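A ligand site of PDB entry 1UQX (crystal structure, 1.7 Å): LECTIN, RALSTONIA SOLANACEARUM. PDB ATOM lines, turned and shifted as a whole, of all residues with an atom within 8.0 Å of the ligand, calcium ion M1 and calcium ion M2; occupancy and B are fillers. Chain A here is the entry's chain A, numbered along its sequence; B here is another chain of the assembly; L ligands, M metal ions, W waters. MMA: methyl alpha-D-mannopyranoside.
The side-chain carboxylate (OD2) of Asp 95 lies within hydrogen-bond range of an oxygen (O6) of the ligand (2.6 Å). An oxygen (O5) of the ligand is in hydrogen-bond range of the backbone NH (N) of Ala 23 (2.9 Å). An oxygen (O6) of the ligand is in hydrogen-bond range of the backbone NH of Asn 24 (3.1 Å).
The side-chain carboxylate of Asp 103 sits close to the backbone NH of Asp 95 (2.8 Å). The side-chain carboxylate (OE1) of Glu 94 lies close to the backbone NH (N) of Asn 99, 3.3 Å away. N of Tyr 101 sits close to OE1 of Glu 94. The backbone carbonyl oxygen of Thr 45 sits at hydrogen-bond distance from the backbone NH of Gly 113 of chain B, 2.8 Å away. N of Asn 102 sits at hydrogen-bond distance from O of Ser 93, at 3.4 Å. NE2 of Gln 26 sits at hydrogen-bond distance from OD2 of Asp 95, at 3.0 Å. The backbone carbonyl oxygen of Asn 24 is in hydrogen-bond range of the side-chain amide nitrogen of Gln 26 (3.0 Å). The backbone carbonyl oxygen (O) of Gly 44 lies within hydrogen-bond range of the backbone NH (N) of Ala 22, 2.8 Å away.
Ala 22 touches the ligand. Within 4 Å of the ligand: Asn 21, Ala 22, Ala 23, Asn 24, Glu 94, Asp 95, Asp 98, Asp 100, Asp 103 and Gly 113 of chain B.
Of the 27 residues printed, 5 come within 4 Å of calcium ion M1.
Of the 27 residues printed, 4 come within 4 Å of calcium ion M2. The nearest printed residue that does not touch calcium ion M2 is Asp 95 (4.1 Å).
Calcium ion M1 is bound by O of Asn 21 (2.3 Å), OD1 of Asp 103 (2.4 Å), O of Gly 113 of chain B (2.4 Å), OD1 of Asn 102 (2.4 Å), OD2 of Asp 100 (2.4 Å), O3 of the ligand (2.5 Å) and O2 of the ligand (2.5 Å). Calcium ion M1 has seven donor atoms within binding distance. Slightly farther from calcium ion M1 lies OD1 of Asp 100 (3.1 Å).
The side-chain carboxylate (OD1) of Asp 98 is bound to calcium ion M2. Calcium ion M2 is bound by OE2 of Glu 94, 2.4 Å away. Calcium ion M2 is bound by OD1 of Asp 100 (2.4 Å). Calcium ion M2 is bound by the side-chain carboxylate (OD2) of Asp 103, at 2.4 Å. OE1 of Glu 94 binds calcium ion M2 (2.5 Å). An oxygen (O3) of the ligand is bound to calcium ion M2, 2.5 Å away. O4 of the ligand binds calcium ion M2, 2.5 Å away. Calcium ion M2 is bound by OD1 of Asp 103 (2.7 Å). Calcium ion M2 has eight donor atoms within binding distance.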
ATOM      1  N   ALA A  20       3.548 -12.653   0.660  1.00  0.00           N
ATOM      2  CA  ALA A  20       4.967 -12.322   0.727  1.00  0.00           C
ATOM      3  C   ALA A  20       5.239 -10.847   0.641  1.00  0.00           C
ATOM      4  O   ALA A  20       4.549 -10.076  -0.053  1.00  0.00           O
ATOM      5  CB  ALA A  20       5.724 -13.029  -0.396  1.00  0.00           C
ATOM      6  N   ASN A  21       6.255 -10.427   1.355  1.00  0.00           N
ATOM      7  CA  ASN A  21       6.886  -9.092   1.221  1.00  0.00           C
ATOM      8  C   ASN A  21       8.401  -9.332   1.334  1.00  0.00           C
ATOM      9  O   ASN A  21       9.054  -9.041   2.355  1.00  0.00           O
ATOM     10  CB  ASN A  21       6.427  -8.106   2.270  1.00  0.00           C
ATOM     11  CG  ASN A  21       4.969  -7.754   2.123  1.00  0.00           C
ATOM     12  OD1 ASN A  21       4.606  -6.896   1.353  1.00  0.00           O
ATOM     13  ND2 ASN A  21       4.124  -8.435   2.903  1.00  0.00           N
ATOM     14  N   ALA A  22       8.936  -9.932   0.300  1.00  0.00           N
ATOM     15  CA  ALA A  22      10.292 -10.507   0.348  1.00  0.00           C
ATOM     16  C   ALA A  22      10.900 -10.707  -1.007  1.00  0.00           C
ATOM     17  O   ALA A  22      10.207 -11.093  -1.948  1.00  0.00           O
ATOM     18  CB  ALA A  22      10.271 -11.878   1.085  1.00  0.00           C
ATOM     19  N   ALA A  23      12.221 -10.533  -1.119  1.00  0.00           N
ATOM     20  CA  ALA A  23      12.927 -10.948  -2.329  1.00  0.00           C
ATOM     21  C   ALA A  23      13.086 -12.456  -2.428  1.00  0.00           C
ATOM     22  O   ALA A  23      13.116 -13.004  -3.527  1.00  0.00           O
ATOM     23  CB  ALA A  23      14.301 -10.278  -2.444  1.00  0.00           C
ATOM     24  N   ASN A  24      13.218 -13.122  -1.300  1.00  0.00           N
ATOM     25  CA  ASN A  24      13.373 -14.572  -1.249  1.00  0.00           C
ATOM     26  C   ASN A  24      12.053 -15.333  -1.268  1.00  0.00           C
ATOM     27  O   ASN A  24      11.017 -14.828  -0.778  1.00  0.00           O
ATOM     28  CB  ASN A  24      14.211 -14.994  -0.046  1.00  0.00           C
ATOM     29  CG  ASN A  24      15.672 -14.556  -0.165  1.00  0.00           C
ATOM     30  OD1 ASN A  24      16.174 -14.393  -1.270  1.00  0.00           O
ATOM     31  ND2 ASN A  24      16.330 -14.400   0.954  1.00  0.00           N
ATOM     32  N   THR A  25      12.079 -16.507  -1.906  1.00  0.00           N
ATOM     33  CA  THR A  25      10.907 -17.378  -1.957  1.00  0.00           C
ATOM     34  C   THR A  25      10.527 -17.865  -0.565  1.00  0.00           C
ATOM     35  O   THR A  25      11.302 -18.558   0.103  1.00  0.00           O
ATOM     36  CB  THR A  25      11.203 -18.561  -2.859  1.00  0.00           C
ATOM     37  OG1 THR A  25      11.513 -18.021  -4.158  1.00  0.00           O
ATOM     38  CG2 THR A  25       9.985 -19.428  -3.012  1.00  0.00           C
ATOM     39  N   GLN A  26       9.291 -17.534  -0.180  1.00  0.00           N
ATOM     40  CA  GLN A  26       8.728 -17.981   1.078  1.00  0.00           C
ATOM     41  C   GLN A  26       8.001 -19.309   0.883  1.00  0.00           C
ATOM     42  O   GLN A  26       7.284 -19.473  -0.095  1.00  0.00           O
ATOM     43  CB  GLN A  26       7.734 -16.934   1.584  1.00  0.00           C
ATOM     44  CG  GLN A  26       8.282 -15.518   1.611  1.00  0.00           C
ATOM     45  CD  GLN A  26       9.360 -15.360   2.640  1.00  0.00           C
ATOM     46  OE1 GLN A  26       9.117 -15.644   3.823  1.00  0.00           O
ATOM     47  NE2 GLN A  26      10.560 -14.931   2.207  1.00  0.00           N
ATOM     48  N   SER A  43       7.302 -15.208  -3.830  1.00  0.00           N
ATOM     49  CA  SER A  43       8.058 -14.022  -3.443  1.00  0.00           C
ATOM     50  C   SER A  43       7.407 -12.799  -4.076  1.00  0.00           C
ATOM     51  O   SER A  43       6.465 -12.897  -4.871  1.00  0.00           O
ATOM     52  CB  SER A  43       9.507 -14.135  -3.901  1.00  0.00           C
ATOM     53  OG  SER A  43       9.576 -14.168  -5.308  1.00  0.00           O
ATOM     54  N   GLY A  44       7.907 -11.636  -3.698  1.00  0.00           N
ATOM     55  CA  GLY A  44       7.378 -10.370  -4.174  1.00  0.00           C
ATOM     56  C   GLY A  44       7.351  -9.419  -3.008  1.00  0.00           C
ATOM     57  O   GLY A  44       7.104  -9.856  -1.877  1.00  0.00           O
ATOM     58  N   THR A  45       7.615  -8.144  -3.268  1.00  0.00           N
ATOM     59  CA  THR A  45       7.782  -7.195  -2.166  1.00  0.00           C
ATOM     60  C   THR A  45       6.602  -6.274  -1.966  1.00  0.00           C
ATOM     61  O   THR A  45       6.664  -5.409  -1.084  1.00  0.00           O
ATOM     62  CB  THR A  45       9.064  -6.357  -2.341  1.00  0.00           C
ATOM     63  OG1 THR A  45       9.085  -5.797  -3.678  1.00  0.00           O
ATOM     64  CG2 THR A  45      10.283  -7.224  -2.226  1.00  0.00           C
ATOM     65  N   SER A  46       5.530  -6.454  -2.751  1.00  0.00           N
ATOM     66  CA  SER A  46       4.310  -5.666  -2.596  1.00  0.00           C
ATOM     67  C   SER A  46       3.103  -6.523  -2.202  1.00  0.00           C
ATOM     68  O   SER A  46       2.143  -6.605  -2.938  1.00  0.00           O
ATOM     69  CB  SER A  46       4.002  -4.928  -3.898  1.00  0.00           C
ATOM     70  OG  SER A  46       4.982  -3.942  -4.136  1.00  0.00           O
ATOM     71  N   VAL A  68      12.538 -20.392   4.259  1.00  0.00           N
ATOM     72  CA  VAL A  68      13.057 -19.993   2.965  1.00  0.00           C
ATOM     73  C   VAL A  68      14.115 -21.049   2.613  1.00  0.00           C
ATOM     74  O   VAL A  68      15.113 -21.166   3.328  1.00  0.00           O
ATOM     75  CB  VAL A  68      13.721 -18.627   3.060  1.00  0.00           C
ATOM     76  CG1 VAL A  68      14.464 -18.369   1.717  1.00  0.00           C
ATOM     77  CG2 VAL A  68      12.697 -17.600   3.376  1.00  0.00           C
ATOM     78  N   SER A  93       6.841 -12.950   9.872  1.00  0.00           N
ATOM     79  CA  SER A  93       8.084 -13.682   9.939  1.00  0.00           C
ATOM     80  C   SER A  93       9.206 -12.848   9.329  1.00  0.00           C
ATOM     81  O   SER A  93       8.976 -12.027   8.466  1.00  0.00           O
ATOM     82  CB  SER A  93       7.976 -14.990   9.170  1.00  0.00           C
ATOM     83  OG  SER A  93       7.734 -14.814   7.777  1.00  0.00           O
ATOM     84  N   GLU A  94      10.416 -13.135   9.806  1.00  0.00           N
ATOM     85  CA  GLU A  94      11.626 -12.459   9.358  1.00  0.00           C
ATOM     86  C   GLU A  94      12.630 -13.508   8.862  1.00  0.00           C
ATOM     87  O   GLU A  94      13.017 -14.415   9.592  1.00  0.00           O
ATOM     88  CB  GLU A  94      12.229 -11.662  10.504  1.00  0.00           C
ATOM     89  CG  GLU A  94      13.504 -10.886  10.149  1.00  0.00           C
ATOM     90  CD  GLU A  94      13.344 -10.068   8.899  1.00  0.00           C
ATOM     91  OE1 GLU A  94      12.380  -9.268   8.837  1.00  0.00           O
ATOM     92  OE2 GLU A  94      14.129 -10.220   7.924  1.00  0.00           O
ATOM     93  N   ASP A  95      13.019 -13.371   7.595  1.00  0.00           N
ATOM     94  CA  ASP A  95      13.947 -14.300   6.947  1.00  0.00           C
ATOM     95  C   ASP A  95      15.390 -13.801   6.884  1.00  0.00           C
ATOM     96  O   ASP A  95      16.279 -14.496   6.362  1.00  0.00           O
ATOM     97  CB  ASP A  95      13.454 -14.657   5.560  1.00  0.00           C
ATOM     98  CG  ASP A  95      13.550 -13.534   4.553  1.00  0.00           C
ATOM     99  OD1 ASP A  95      14.204 -12.479   4.836  1.00  0.00           O
ATOM    100  OD2 ASP A  95      12.955 -13.629   3.433  1.00  0.00           O
ATOM    101  N   GLY A  96      15.605 -12.604   7.428  1.00  0.00           N
ATOM    102  CA  GLY A  96      16.836 -11.852   7.227  1.00  0.00           C
ATOM    103  C   GLY A  96      17.217 -11.001   8.404  1.00  0.00           C
ATOM    104  O   GLY A  96      17.112 -11.434   9.598  1.00  0.00           O
ATOM    105  N   THR A  97      17.667  -9.786   8.107  1.00  0.00           N
ATOM    106  CA  THR A  97      18.239  -8.911   9.110  1.00  0.00           C
ATOM    107  C   THR A  97      17.547  -7.570   9.257  1.00  0.00           C
ATOM    108  O   THR A  97      17.854  -6.835  10.200  1.00  0.00           O
ATOM    109  CB  THR A  97      19.735  -8.636   8.783  1.00  0.00           C
ATOM    110  OG1 THR A  97      19.810  -8.103   7.449  1.00  0.00           O
ATOM    111  CG2 THR A  97      20.619  -9.897   8.840  1.00  0.00           C
ATOM    112  N   ASP A  98      16.679  -7.172   8.343  1.00  0.00           N
ATOM    113  CA  ASP A  98      16.055  -5.862   8.422  1.00  0.00           C
ATOM    114  C   ASP A  98      14.905  -5.762   9.455  1.00  0.00           C
ATOM    115  O   ASP A  98      14.482  -4.671   9.767  1.00  0.00           O
ATOM    116  CB  ASP A  98      15.600  -5.293   7.082  1.00  0.00           C
ATOM    117  CG  ASP A  98      14.461  -6.066   6.452  1.00  0.00           C
ATOM    118  OD1 ASP A  98      14.140  -7.198   6.936  1.00  0.00           O
ATOM    119  OD2 ASP A  98      13.894  -5.616   5.411  1.00  0.00           O
ATOM    120  N   ASN A  99      14.442  -6.907   9.962  1.00  0.00           N
ATOM    121  CA  ASN A  99      13.432  -6.975  11.022  1.00  0.00           C
ATOM    122  C   ASN A  99      12.159  -6.227  10.693  1.00  0.00           C
ATOM    123  O   ASN A  99      11.548  -5.576  11.573  1.00  0.00           O
ATOM    124  CB  ASN A  99      14.052  -6.571  12.357  1.00  0.00           C
ATOM    125  CG  ASN A  99      15.158  -7.509  12.779  1.00  0.00           C
ATOM    126  OD1 ASN A  99      15.247  -8.670  12.290  1.00  0.00           O
ATOM    127  ND2 ASN A  99      16.065  -7.002  13.600  1.00  0.00           N
ATOM    128  N   ASP A 100      11.727  -6.329   9.440  1.00  0.00           N
ATOM    129  CA  ASP A 100      10.387  -5.880   9.083  1.00  0.00           C
ATOM    130  C   ASP A 100       9.291  -6.885   9.406  1.00  0.00           C
ATOM    131  O   ASP A 100       8.094  -6.514   9.496  1.00  0.00           O
ATOM    132  CB  ASP A 100      10.294  -5.313   7.658  1.00  0.00           C
ATOM    133  CG  ASP A 100      10.622  -6.299   6.576  1.00  0.00           C
ATOM    134  OD1 ASP A 100      10.947  -7.507   6.862  1.00  0.00           O
ATOM    135  OD2 ASP A 100      10.498  -5.900   5.385  1.00  0.00           O
ATOM    136  N   TYR A 101       9.667  -8.164   9.584  1.00  0.00           N
ATOM    137  CA  TYR A 101       8.722  -9.206  10.042  1.00  0.00           C
ATOM    138  C   TYR A 101       7.517  -9.382   9.119  1.00  0.00           C
ATOM    139  O   TYR A 101       6.493  -9.910   9.526  1.00  0.00           O
ATOM    140  CB  TYR A 101       8.316  -8.961  11.538  1.00  0.00           C
ATOM    141  CG  TYR A 101       9.405  -9.550  12.427  1.00  0.00           C
ATOM    142  CD1 TYR A 101       9.411 -10.884  12.717  1.00  0.00           C
ATOM    143  CD2 TYR A 101      10.469  -8.777  12.855  1.00  0.00           C
ATOM    144  CE1 TYR A 101      10.468 -11.448  13.446  1.00  0.00           C
ATOM    145  CE2 TYR A 101      11.492  -9.324  13.540  1.00  0.00           C
ATOM    146  CZ  TYR A 101      11.491 -10.647  13.858  1.00  0.00           C
ATOM    147  OH  TYR A 101      12.569 -11.194  14.560  1.00  0.00           O
ATOM    148  N   ASN A 102       7.656  -8.980   7.848  1.00  0.00           N
ATOM    149  CA  ASN A 102       6.557  -9.055   6.901  1.00  0.00           C
ATOM    150  C   ASN A 102       6.846 -10.037   5.768  1.00  0.00           C
ATOM    151  O   ASN A 102       6.134 -10.082   4.768  1.00  0.00           O
ATOM    152  CB  ASN A 102       6.214  -7.649   6.354  1.00  0.00           C
ATOM    153  CG  ASN A 102       7.292  -7.124   5.457  1.00  0.00           C
ATOM    154  OD1 ASN A 102       8.272  -7.841   5.246  1.00  0.00           O
ATOM    155  ND2 ASN A 102       7.144  -5.906   4.928  1.00  0.00           N
ATOM    156  N   ASP A 103       7.936 -10.800   5.895  1.00  0.00           N
ATOM    157  CA  ASP A 103       8.485 -11.505   4.733  1.00  0.00           C
ATOM    158  C   ASP A 103       7.538 -12.573   4.222  1.00  0.00           C
ATOM    159  O   ASP A 103       7.256 -12.680   3.013  1.00  0.00           O
ATOM    160  CB  ASP A 103       9.878 -12.057   5.032  1.00  0.00           C
ATOM    161  CG  ASP A 103      10.853 -10.995   5.417  1.00  0.00           C
ATOM    162  OD1 ASP A 103      10.845  -9.894   4.776  1.00  0.00           O
ATOM    163  OD2 ASP A 103      11.705 -11.199   6.332  1.00  0.00           O
ATOM    164  N   GLY A 104       6.998 -13.362   5.157  1.00  0.00           N
ATOM    165  CA  GLY A 104       5.967 -14.364   4.872  1.00  0.00           C
ATOM    166  C   GLY A 104       4.903 -14.197   5.965  1.00  0.00           C
ATOM    167  O   GLY A 104       5.223 -14.216   7.164  1.00  0.00           O
ATOM    168  N   PRO B 111       4.037  -2.437   7.352  1.00  0.00           N
ATOM    169  CA  PRO B 111       4.557  -1.992   6.056  1.00  0.00           C
ATOM    170  C   PRO B 111       4.820  -3.154   5.130  1.00  0.00           C
ATOM    171  O   PRO B 111       4.880  -4.297   5.530  1.00  0.00           O
ATOM    172  CB  PRO B 111       5.869  -1.331   6.456  1.00  0.00           C
ATOM    173  CG  PRO B 111       6.350  -2.145   7.612  1.00  0.00           C
ATOM    174  CD  PRO B 111       5.091  -2.465   8.382  1.00  0.00           C
ATOM    175  N   LEU B 112       4.950  -2.818   3.856  1.00  0.00           N
ATOM    176  CA  LEU B 112       5.246  -3.770   2.830  1.00  0.00           C
ATOM    177  C   LEU B 112       6.741  -3.693   2.577  1.00  0.00           C
ATOM    178  O   LEU B 112       7.463  -3.089   3.363  1.00  0.00           O
ATOM    179  CB  LEU B 112       4.388  -3.484   1.603  1.00  0.00           C
ATOM    180  CG  LEU B 112       2.887  -3.309   1.797  1.00  0.00           C
ATOM    181  CD1 LEU B 112       2.203  -3.168   0.422  1.00  0.00           C
ATOM    182  CD2 LEU B 112       2.345  -4.515   2.544  1.00  0.00           C
ATOM    183  N   GLY B 113       7.214  -4.315   1.480  1.00  0.00           N
ATOM    184  CA  GLY B 113       8.650  -4.235   1.137  1.00  0.00           C
ATOM    185  C   GLY B 113       9.516  -5.412   1.557  1.00  0.00           C
ATOM    186  O   GLY B 113       9.248  -5.985   2.665  1.00  0.00           O
ATOM    187  OXT GLY B 113      10.474  -5.773   0.794  1.00  0.00           O
HETATM  188  C1  MMA L   1      13.970  -7.889   0.905  1.00  0.00           C
HETATM  189  C2  MMA L   1      13.045  -7.365   2.027  1.00  0.00           C
HETATM  190  C3  MMA L   1      13.587  -7.967   3.328  1.00  0.00           C
HETATM  191  C4  MMA L   1      13.720  -9.506   3.239  1.00  0.00           C
HETATM  192  C5  MMA L   1      14.613  -9.838   2.006  1.00  0.00           C
HETATM  193  C6  MMA L   1      14.847 -11.345   1.808  1.00  0.00           C
HETATM  194  C7  MMA L   1      15.999  -7.475  -0.325  1.00  0.00           C
HETATM  195  O1  MMA L   1      15.208  -7.190   0.884  1.00  0.00           O
HETATM  196  O2  MMA L   1      11.684  -7.714   1.804  1.00  0.00           O
HETATM  197  O3  MMA L   1      12.700  -7.561   4.355  1.00  0.00           O
HETATM  198  O4  MMA L   1      14.176  -9.942   4.523  1.00  0.00           O
HETATM  199  O5  MMA L   1      14.034  -9.296   0.826  1.00  0.00           O
HETATM  200  O6  MMA L   1      13.602 -11.963   1.547  1.00  0.00           O
HETATM  201 CA    CA M   1      10.257  -7.787   3.868  1.00  0.00          CA
HETATM  202 CA    CA M   2      12.738  -9.015   6.409  1.00  0.00          CA
HETATM  203  O   HOH W   1      16.689  -8.756   5.492  1.00  0.00           O
HETATM  204  O   HOH W   2      16.983  -5.176   2.912  1.00  0.00           O
